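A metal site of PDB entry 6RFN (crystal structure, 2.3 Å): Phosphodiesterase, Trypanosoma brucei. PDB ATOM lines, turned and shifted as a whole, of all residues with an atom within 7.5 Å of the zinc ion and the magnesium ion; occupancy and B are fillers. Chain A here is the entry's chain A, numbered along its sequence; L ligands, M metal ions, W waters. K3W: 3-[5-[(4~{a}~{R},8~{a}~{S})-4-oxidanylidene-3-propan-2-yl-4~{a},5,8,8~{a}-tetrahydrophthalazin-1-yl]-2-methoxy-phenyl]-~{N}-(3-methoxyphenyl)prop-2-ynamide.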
ATOM      1  N   TYR A 110      -9.015  -2.546   3.944  1.00  0.00           N
ATOM      2  CA  TYR A 110      -9.777  -2.791   2.675  1.00  0.00           C
ATOM      3  C   TYR A 110     -10.143  -1.488   1.951  1.00  0.00           C
ATOM      4  O   TYR A 110      -9.756  -1.373   0.771  1.00  0.00           O
ATOM      5  CB  TYR A 110     -11.055  -3.617   2.890  1.00  0.00           C
ATOM      6  CG  TYR A 110     -11.758  -3.987   1.609  1.00  0.00           C
ATOM      7  CD1 TYR A 110     -11.413  -5.113   0.880  1.00  0.00           C
ATOM      8  CD2 TYR A 110     -12.792  -3.205   1.105  1.00  0.00           C
ATOM      9  CE1 TYR A 110     -12.068  -5.477  -0.285  1.00  0.00           C
ATOM     10  CE2 TYR A 110     -13.460  -3.548  -0.064  1.00  0.00           C
ATOM     11  CZ  TYR A 110     -13.104  -4.687  -0.768  1.00  0.00           C
ATOM     12  OH  TYR A 110     -13.776  -4.992  -1.918  1.00  0.00           O
ATOM     13  N   HIS A 111     -10.860  -0.550   2.580  1.00  0.00           N
ATOM     14  CA  HIS A 111     -11.368   0.654   1.880  1.00  0.00           C
ATOM     15  C   HIS A 111     -10.286   1.736   1.861  1.00  0.00           C
ATOM     16  O   HIS A 111     -10.564   2.849   2.300  1.00  0.00           O
ATOM     17  CB  HIS A 111     -12.658   1.128   2.516  1.00  0.00           C
ATOM     18  CG  HIS A 111     -13.783   0.182   2.339  1.00  0.00           C
ATOM     19  ND1 HIS A 111     -14.260  -0.572   3.379  1.00  0.00           N
ATOM     20  CD2 HIS A 111     -14.574  -0.071   1.280  1.00  0.00           C
ATOM     21  CE1 HIS A 111     -15.288  -1.270   2.963  1.00  0.00           C
ATOM     22  NE2 HIS A 111     -15.505  -0.986   1.679  1.00  0.00           N
ATOM     23  N   HIS A 115      -8.200  -0.164  -3.099  1.00  0.00           N
ATOM     24  CA  HIS A 115      -9.548  -0.679  -3.430  1.00  0.00           C
ATOM     25  C   HIS A 115     -10.141   0.125  -4.588  1.00  0.00           C
ATOM     26  O   HIS A 115     -10.733  -0.481  -5.490  1.00  0.00           O
ATOM     27  CB  HIS A 115     -10.452  -0.638  -2.220  1.00  0.00           C
ATOM     28  CG  HIS A 115     -11.903  -0.747  -2.568  1.00  0.00           C
ATOM     29  ND1 HIS A 115     -12.460  -1.917  -3.044  1.00  0.00           N
ATOM     30  CD2 HIS A 115     -12.895   0.149  -2.475  1.00  0.00           C
ATOM     31  CE1 HIS A 115     -13.740  -1.721  -3.217  1.00  0.00           C
ATOM     32  NE2 HIS A 115     -14.030  -0.469  -2.868  1.00  0.00           N
ATOM     33  N   VAL A 116      -9.972   1.439  -4.597  1.00  0.00           N
ATOM     34  CA  VAL A 116     -10.700   2.288  -5.596  1.00  0.00           C
ATOM     35  C   VAL A 116      -9.934   2.217  -6.921  1.00  0.00           C
ATOM     36  O   VAL A 116     -10.576   2.254  -8.001  1.00  0.00           O
ATOM     37  CB  VAL A 116     -10.944   3.714  -5.048  1.00  0.00           C
ATOM     38  CG1 VAL A 116     -11.613   3.705  -3.692  1.00  0.00           C
ATOM     39  CG2 VAL A 116      -9.684   4.548  -4.977  1.00  0.00           C
ATOM     40  N   VAL A 119     -11.207  -0.946  -8.368  1.00  0.00           N
ATOM     41  CA  VAL A 119     -12.564  -0.766  -8.961  1.00  0.00           C
ATOM     42  C   VAL A 119     -12.425  -0.074 -10.307  1.00  0.00           C
ATOM     43  O   VAL A 119     -13.109  -0.506 -11.250  1.00  0.00           O
ATOM     44  CB  VAL A 119     -13.529  -0.011  -8.029  1.00  0.00           C
ATOM     45  CG1 VAL A 119     -14.824   0.409  -8.742  1.00  0.00           C
ATOM     46  CG2 VAL A 119     -13.831  -0.856  -6.789  1.00  0.00           C
ATOM     47  N   ALA A 148     -14.811   5.857 -10.056  1.00  0.00           N
ATOM     48  CA  ALA A 148     -14.196   4.702  -9.371  1.00  0.00           C
ATOM     49  C   ALA A 148     -13.258   5.243  -8.308  1.00  0.00           C
ATOM     50  O   ALA A 148     -13.225   4.711  -7.193  1.00  0.00           O
ATOM     51  CB  ALA A 148     -13.489   3.844 -10.377  1.00  0.00           C
ATOM     52  N   HIS A 151     -15.210   6.946  -5.041  1.00  0.00           N
ATOM     53  CA  HIS A 151     -16.488   6.329  -4.596  1.00  0.00           C
ATOM     54  C   HIS A 151     -16.404   5.902  -3.114  1.00  0.00           C
ATOM     55  O   HIS A 151     -17.463   5.606  -2.557  1.00  0.00           O
ATOM     56  CB  HIS A 151     -16.895   5.190  -5.552  1.00  0.00           C
ATOM     57  CG  HIS A 151     -16.336   3.875  -5.151  1.00  0.00           C
ATOM     58  ND1 HIS A 151     -15.057   3.487  -5.490  1.00  0.00           N
ATOM     59  CD2 HIS A 151     -16.828   2.914  -4.337  1.00  0.00           C
ATOM     60  CE1 HIS A 151     -14.795   2.322  -4.939  1.00  0.00           C
ATOM     61  NE2 HIS A 151     -15.852   1.965  -4.193  1.00  0.00           N
ATOM     62  N   ASP A 152     -15.228   5.859  -2.503  1.00  0.00           N
ATOM     63  CA  ASP A 152     -15.056   5.531  -1.055  1.00  0.00           C
ATOM     64  C   ASP A 152     -14.234   6.591  -0.290  1.00  0.00           C
ATOM     65  O   ASP A 152     -13.698   6.251   0.782  1.00  0.00           O
ATOM     66  CB  ASP A 152     -14.394   4.168  -0.858  1.00  0.00           C
ATOM     67  CG  ASP A 152     -15.385   3.025  -1.020  1.00  0.00           C
ATOM     68  OD1 ASP A 152     -16.550   3.181  -0.563  1.00  0.00           O
ATOM     69  OD2 ASP A 152     -14.977   1.991  -1.658  1.00  0.00           O
ATOM     70  N   LEU A 153     -14.177   7.849  -0.750  1.00  0.00           N
ATOM     71  CA  LEU A 153     -13.308   8.897  -0.162  1.00  0.00           C
ATOM     72  C   LEU A 153     -13.510   9.037   1.359  1.00  0.00           C
ATOM     73  O   LEU A 153     -14.642   9.221   1.812  1.00  0.00           O
ATOM     74  CB  LEU A 153     -13.576  10.252  -0.807  1.00  0.00           C
ATOM     75  CG  LEU A 153     -13.052  10.409  -2.229  1.00  0.00           C
ATOM     76  CD1 LEU A 153     -13.687  11.629  -2.854  1.00  0.00           C
ATOM     77  CD2 LEU A 153     -11.527  10.475  -2.255  1.00  0.00           C
ATOM     78  N   HIS A 155     -13.000   6.958   3.820  1.00  0.00           N
ATOM     79  CA  HIS A 155     -13.624   5.780   4.472  1.00  0.00           C
ATOM     80  C   HIS A 155     -12.793   5.465   5.711  1.00  0.00           C
ATOM     81  O   HIS A 155     -11.547   5.518   5.587  1.00  0.00           O
ATOM     82  CB  HIS A 155     -13.685   4.587   3.497  1.00  0.00           C
ATOM     83  CG  HIS A 155     -14.723   3.575   3.842  1.00  0.00           C
ATOM     84  ND1 HIS A 155     -14.609   2.776   4.941  1.00  0.00           N
ATOM     85  CD2 HIS A 155     -15.909   3.260   3.270  1.00  0.00           C
ATOM     86  CE1 HIS A 155     -15.689   1.995   5.027  1.00  0.00           C
ATOM     87  NE2 HIS A 155     -16.497   2.265   3.997  1.00  0.00           N
ATOM     88  N   LEU A 183     -22.091   7.112   4.645  1.00  0.00           N
ATOM     89  CA  LEU A 183     -20.759   7.174   3.995  1.00  0.00           C
ATOM     90  C   LEU A 183     -20.879   7.718   2.568  1.00  0.00           C
ATOM     91  O   LEU A 183     -20.005   8.516   2.154  1.00  0.00           O
ATOM     92  CB  LEU A 183     -20.143   5.787   3.997  1.00  0.00           C
ATOM     93  CG  LEU A 183     -19.578   5.358   5.337  1.00  0.00           C
ATOM     94  CD1 LEU A 183     -19.419   3.850   5.408  1.00  0.00           C
ATOM     95  CD2 LEU A 183     -18.255   6.060   5.589  1.00  0.00           C
ATOM     96  N   GLU A 184     -21.909   7.311   1.831  1.00  0.00           N
ATOM     97  CA  GLU A 184     -21.961   7.619   0.381  1.00  0.00           C
ATOM     98  C   GLU A 184     -22.099   9.131   0.234  1.00  0.00           C
ATOM     99  O   GLU A 184     -21.443   9.709  -0.634  1.00  0.00           O
ATOM    100  CB  GLU A 184     -23.053   6.795  -0.315  1.00  0.00           C
ATOM    101  CG  GLU A 184     -22.785   5.287  -0.311  1.00  0.00           C
ATOM    102  CD  GLU A 184     -22.950   4.502   0.980  1.00  0.00           C
ATOM    103  OE1 GLU A 184     -23.620   5.016   1.923  1.00  0.00           O
ATOM    104  OE2 GLU A 184     -22.397   3.378   1.049  1.00  0.00           O
ATOM    105  N   HIS A 187     -18.768  10.738   0.858  1.00  0.00           N
ATOM    106  CA  HIS A 187     -17.873  10.539  -0.319  1.00  0.00           C
ATOM    107  C   HIS A 187     -18.232  11.611  -1.360  1.00  0.00           C
ATOM    108  O   HIS A 187     -17.336  12.302  -1.829  1.00  0.00           O
ATOM    109  CB  HIS A 187     -17.924   9.126  -0.924  1.00  0.00           C
ATOM    110  CG  HIS A 187     -17.811   7.963   0.020  1.00  0.00           C
ATOM    111  ND1 HIS A 187     -16.841   7.892   0.987  1.00  0.00           N
ATOM    112  CD2 HIS A 187     -18.544   6.835   0.131  1.00  0.00           C
ATOM    113  CE1 HIS A 187     -17.003   6.776   1.673  1.00  0.00           C
ATOM    114  NE2 HIS A 187     -18.026   6.098   1.164  1.00  0.00           N
ATOM    115  N   VAL A 222     -22.241   6.862  -6.988  1.00  0.00           N
ATOM    116  CA  VAL A 222     -21.659   6.689  -5.616  1.00  0.00           C
ATOM    117  C   VAL A 222     -22.797   6.363  -4.621  1.00  0.00           C
ATOM    118  O   VAL A 222     -22.626   5.462  -3.795  1.00  0.00           O
ATOM    119  CB  VAL A 222     -20.937   7.974  -5.169  1.00  0.00           C
ATOM    120  CG1 VAL A 222     -20.485   7.866  -3.730  1.00  0.00           C
ATOM    121  CG2 VAL A 222     -19.793   8.352  -6.106  1.00  0.00           C
ATOM    122  N   THR A 225     -23.880   2.722  -4.498  1.00  0.00           N
ATOM    123  CA  THR A 225     -22.929   1.707  -3.978  1.00  0.00           C
ATOM    124  C   THR A 225     -23.328   1.281  -2.569  1.00  0.00           C
ATOM    125  O   THR A 225     -22.639   0.381  -1.988  1.00  0.00           O
ATOM    126  CB  THR A 225     -21.496   2.255  -3.957  1.00  0.00           C
ATOM    127  OG1 THR A 225     -21.303   3.434  -3.142  1.00  0.00           O
ATOM    128  CG2 THR A 225     -21.052   2.574  -5.358  1.00  0.00           C
ATOM    129  N   ASP A 226     -24.340   1.936  -1.990  1.00  0.00           N
ATOM    130  CA  ASP A 226     -24.895   1.575  -0.668  1.00  0.00           C
ATOM    131  C   ASP A 226     -25.639   0.241  -0.808  1.00  0.00           C
ATOM    132  O   ASP A 226     -26.660   0.205  -1.487  1.00  0.00           O
ATOM    133  CB  ASP A 226     -25.830   2.654  -0.137  1.00  0.00           C
ATOM    134  CG  ASP A 226     -26.432   2.382   1.244  1.00  0.00           C
ATOM    135  OD1 ASP A 226     -26.349   1.249   1.756  1.00  0.00           O
ATOM    136  OD2 ASP A 226     -27.001   3.318   1.781  1.00  0.00           O
ATOM    137  N   MET A 227     -25.166  -0.804  -0.145  1.00  0.00           N
ATOM    138  CA  MET A 227     -25.683  -2.180  -0.385  1.00  0.00           C
ATOM    139  C   MET A 227     -27.098  -2.304   0.162  1.00  0.00           C
ATOM    140  O   MET A 227     -27.734  -3.338  -0.130  1.00  0.00           O
ATOM    141  CB  MET A 227     -24.789  -3.248   0.244  1.00  0.00           C
ATOM    142  CG  MET A 227     -23.500  -3.467  -0.547  1.00  0.00           C
ATOM    143  SD  MET A 227     -23.775  -4.101  -2.238  1.00  0.00           S
ATOM    144  CE  MET A 227     -24.425  -5.716  -1.801  1.00  0.00           C
ATOM    145  N   LEU A 260     -20.575   0.507 -11.673  1.00  0.00           N
ATOM    146  CA  LEU A 260     -19.827   0.855 -10.442  1.00  0.00           C
ATOM    147  C   LEU A 260     -20.167  -0.160  -9.359  1.00  0.00           C
ATOM    148  O   LEU A 260     -19.242  -0.624  -8.702  1.00  0.00           O
ATOM    149  CB  LEU A 260     -20.134   2.285  -9.987  1.00  0.00           C
ATOM    150  CG  LEU A 260     -19.379   2.688  -8.723  1.00  0.00           C
ATOM    151  CD1 LEU A 260     -17.910   2.501  -8.934  1.00  0.00           C
ATOM    152  CD2 LEU A 260     -19.685   4.108  -8.326  1.00  0.00           C
ATOM    153  N   GLY A 263     -18.150  -3.290 -10.250  1.00  0.00           N
ATOM    154  CA  GLY A 263     -16.762  -3.082  -9.819  1.00  0.00           C
ATOM    155  C   GLY A 263     -16.633  -3.249  -8.313  1.00  0.00           C
ATOM    156  O   GLY A 263     -15.672  -3.863  -7.861  1.00  0.00           O
ATOM    157  N   ASP A 264     -17.580  -2.730  -7.536  1.00  0.00           N
ATOM    158  CA  ASP A 264     -17.450  -2.704  -6.057  1.00  0.00           C
ATOM    159  C   ASP A 264     -17.506  -4.133  -5.478  1.00  0.00           C
ATOM    160  O   ASP A 264     -16.775  -4.370  -4.524  1.00  0.00           O
ATOM    161  CB  ASP A 264     -18.501  -1.811  -5.386  1.00  0.00           C
ATOM    162  CG  ASP A 264     -17.995  -1.047  -4.177  1.00  0.00           C
ATOM    163  OD1 ASP A 264     -16.779  -0.805  -4.134  1.00  0.00           O
ATOM    164  OD2 ASP A 264     -18.821  -0.678  -3.313  1.00  0.00           O
ATOM    165  N   ILE A 265     -18.319  -5.045  -6.034  1.00  0.00           N
ATOM    166  CA  ILE A 265     -18.381  -6.457  -5.590  1.00  0.00           C
ATOM    167  C   ILE A 265     -17.646  -7.396  -6.547  1.00  0.00           C
ATOM    168  O   ILE A 265     -17.938  -8.589  -6.554  1.00  0.00           O
ATOM    169  CB  ILE A 265     -19.844  -6.881  -5.330  1.00  0.00           C
ATOM    170  CG1 ILE A 265     -20.726  -6.912  -6.562  1.00  0.00           C
ATOM    171  CG2 ILE A 265     -20.469  -5.980  -4.275  1.00  0.00           C
ATOM    172  CD1 ILE A 265     -22.052  -7.597  -6.258  1.00  0.00           C
HETATM  173  C1  K3W L   1     -24.083 -14.450   3.543  1.00  0.00           C
HETATM  174  C10 K3W L   1     -17.225  -9.514   1.234  1.00  0.00           C
HETATM  175  C11 K3W L   1     -16.375  -9.397   0.101  1.00  0.00           C
HETATM  176  C12 K3W L   1     -14.232 -10.080  -0.707  1.00  0.00           C
HETATM  177  C13 K3W L   1     -16.436  -8.248  -0.692  1.00  0.00           C
HETATM  178  C14 K3W L   1     -17.321  -7.233  -0.390  1.00  0.00           C
HETATM  179  C15 K3W L   1     -18.171  -7.334   0.700  1.00  0.00           C
HETATM  180  C16 K3W L   1     -18.130  -8.487   1.506  1.00  0.00           C
HETATM  181  C17 K3W L   1     -19.168  -6.278   1.063  1.00  0.00           C
HETATM  182  C18 K3W L   1     -22.414  -6.241   2.540  1.00  0.00           C
HETATM  183  C19 K3W L   1     -22.320  -6.824   3.942  1.00  0.00           C
HETATM  184  C2  K3W L   1     -22.556 -12.619   3.094  1.00  0.00           C
HETATM  185  C20 K3W L   1     -22.940  -7.222   1.494  1.00  0.00           C
HETATM  186  C21 K3W L   1     -20.866  -4.318   2.055  1.00  0.00           C
HETATM  187  C22 K3W L   1     -19.480  -3.857   1.641  1.00  0.00           C
HETATM  188  C23 K3W L   1     -19.396  -2.374   1.222  1.00  0.00           C
HETATM  189  C24 K3W L   1     -19.921  -2.154  -0.158  1.00  0.00           C
HETATM  190  C25 K3W L   1     -20.015  -3.104  -1.053  1.00  0.00           C
HETATM  191  C26 K3W L   1     -19.746  -4.550  -0.785  1.00  0.00           C
HETATM  192  C27 K3W L   1     -19.002  -4.830   0.534  1.00  0.00           C
HETATM  193  C28 K3W L   1     -21.356 -13.227   3.495  1.00  0.00           C
HETATM  194  C3  K3W L   1     -22.593 -11.260   2.810  1.00  0.00           C
HETATM  195  C4  K3W L   1     -21.432 -10.510   2.951  1.00  0.00           C
HETATM  196  C5  K3W L   1     -20.243 -11.096   3.324  1.00  0.00           C
HETATM  197  C6  K3W L   1     -20.178 -12.459   3.603  1.00  0.00           C
HETATM  198  C7  K3W L   1     -17.627 -12.756   3.642  1.00  0.00           C
HETATM  199  C8  K3W L   1     -17.360 -11.539   2.933  1.00  0.00           C
HETATM  200  C9  K3W L   1     -17.202 -10.686   2.074  1.00  0.00           C
HETATM  201  N1  K3W L   1     -18.939 -13.004   4.042  1.00  0.00           N
HETATM  202  N2  K3W L   1     -20.118  -6.634   1.865  1.00  0.00           N
HETATM  203  N3  K3W L   1     -21.080  -5.698   2.136  1.00  0.00           N
HETATM  204  O1  K3W L   1     -23.776 -13.212   2.901  1.00  0.00           O
HETATM  205  O2  K3W L   1     -16.708 -13.551   3.788  1.00  0.00           O
HETATM  206  O3  K3W L   1     -15.489 -10.425  -0.120  1.00  0.00           O
HETATM  207  O4  K3W L   1     -21.775  -3.533   2.271  1.00  0.00           O
HETATM  208 ZN    ZN M   1     -16.023   0.450  -2.686  1.00  0.00          ZN
HETATM  209 MG    MG M   2     -18.409   2.396  -0.323  1.00  0.00          MG
HETATM  210  O   HOH W   1     -17.860   1.242  -1.689  1.00  0.00           O
HETATM  211  O   HOH W   2     -16.416  -0.946  -1.069  1.00  0.00           O
HETATM  212  O   HOH W   3     -18.038   0.890   0.876  1.00  0.00           O
HETATM  213  O   HOH W   4     -19.151   3.658  -1.511  1.00  0.00           O
HETATM  214  O   HOH W   5     -19.103   3.321   1.381  1.00  0.00           O
HETATM  215  O   HOH W   6     -20.514   1.670  -0.453  1.00  0.00           O
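Water W2 bridges NE2 of His 111 and OD2 of Asp 264. Water W4 bridges the side-chain hydroxyl (OG1) of Thr 225 (2.7 Å) and the backbone carbonyl oxygen (O) of His 151 (2.8 Å). Water W5 lies within hydrogen-bond range of NE2 of His 187 and OE2 of Glu 184. Water W6 bridges O of Thr 225 (2.9 Å) and OE2 of Glu 184 (3.0 Å).
A ring nitrogen (ND1) of His 151 is in hydrogen-bond range of the backbone carbonyl oxygen (O) of Ala 148 (2.8 Å).
The magnesium ion is bound by water W1 (1.9 Å), water W4 (1.9 Å), water W3 (2.0 Å), OD1 of Asp 152 (2.0 Å), water W5 (2.1 Å) and water W6 (2.2 Å).
Of the 21 residues printed, 4 come within 4 Å of the zinc ion.
The side-chain carboxylate (OD1) of Asp 264 is bound to the zinc ion (2.1 Å). The zinc ion is bound by the side-chain carboxylate (OD2) of Asp 152 (2.1 Å). A ring nitrogen (NE2) of His 151 binds the zinc ion, 2.1 Å away. The zinc ion is bound by water W2 (2.2 Å). The zinc ion is bound by a ring nitrogen (NE2) of His 115 (2.2 Å). Water W1 binds the zinc ion.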
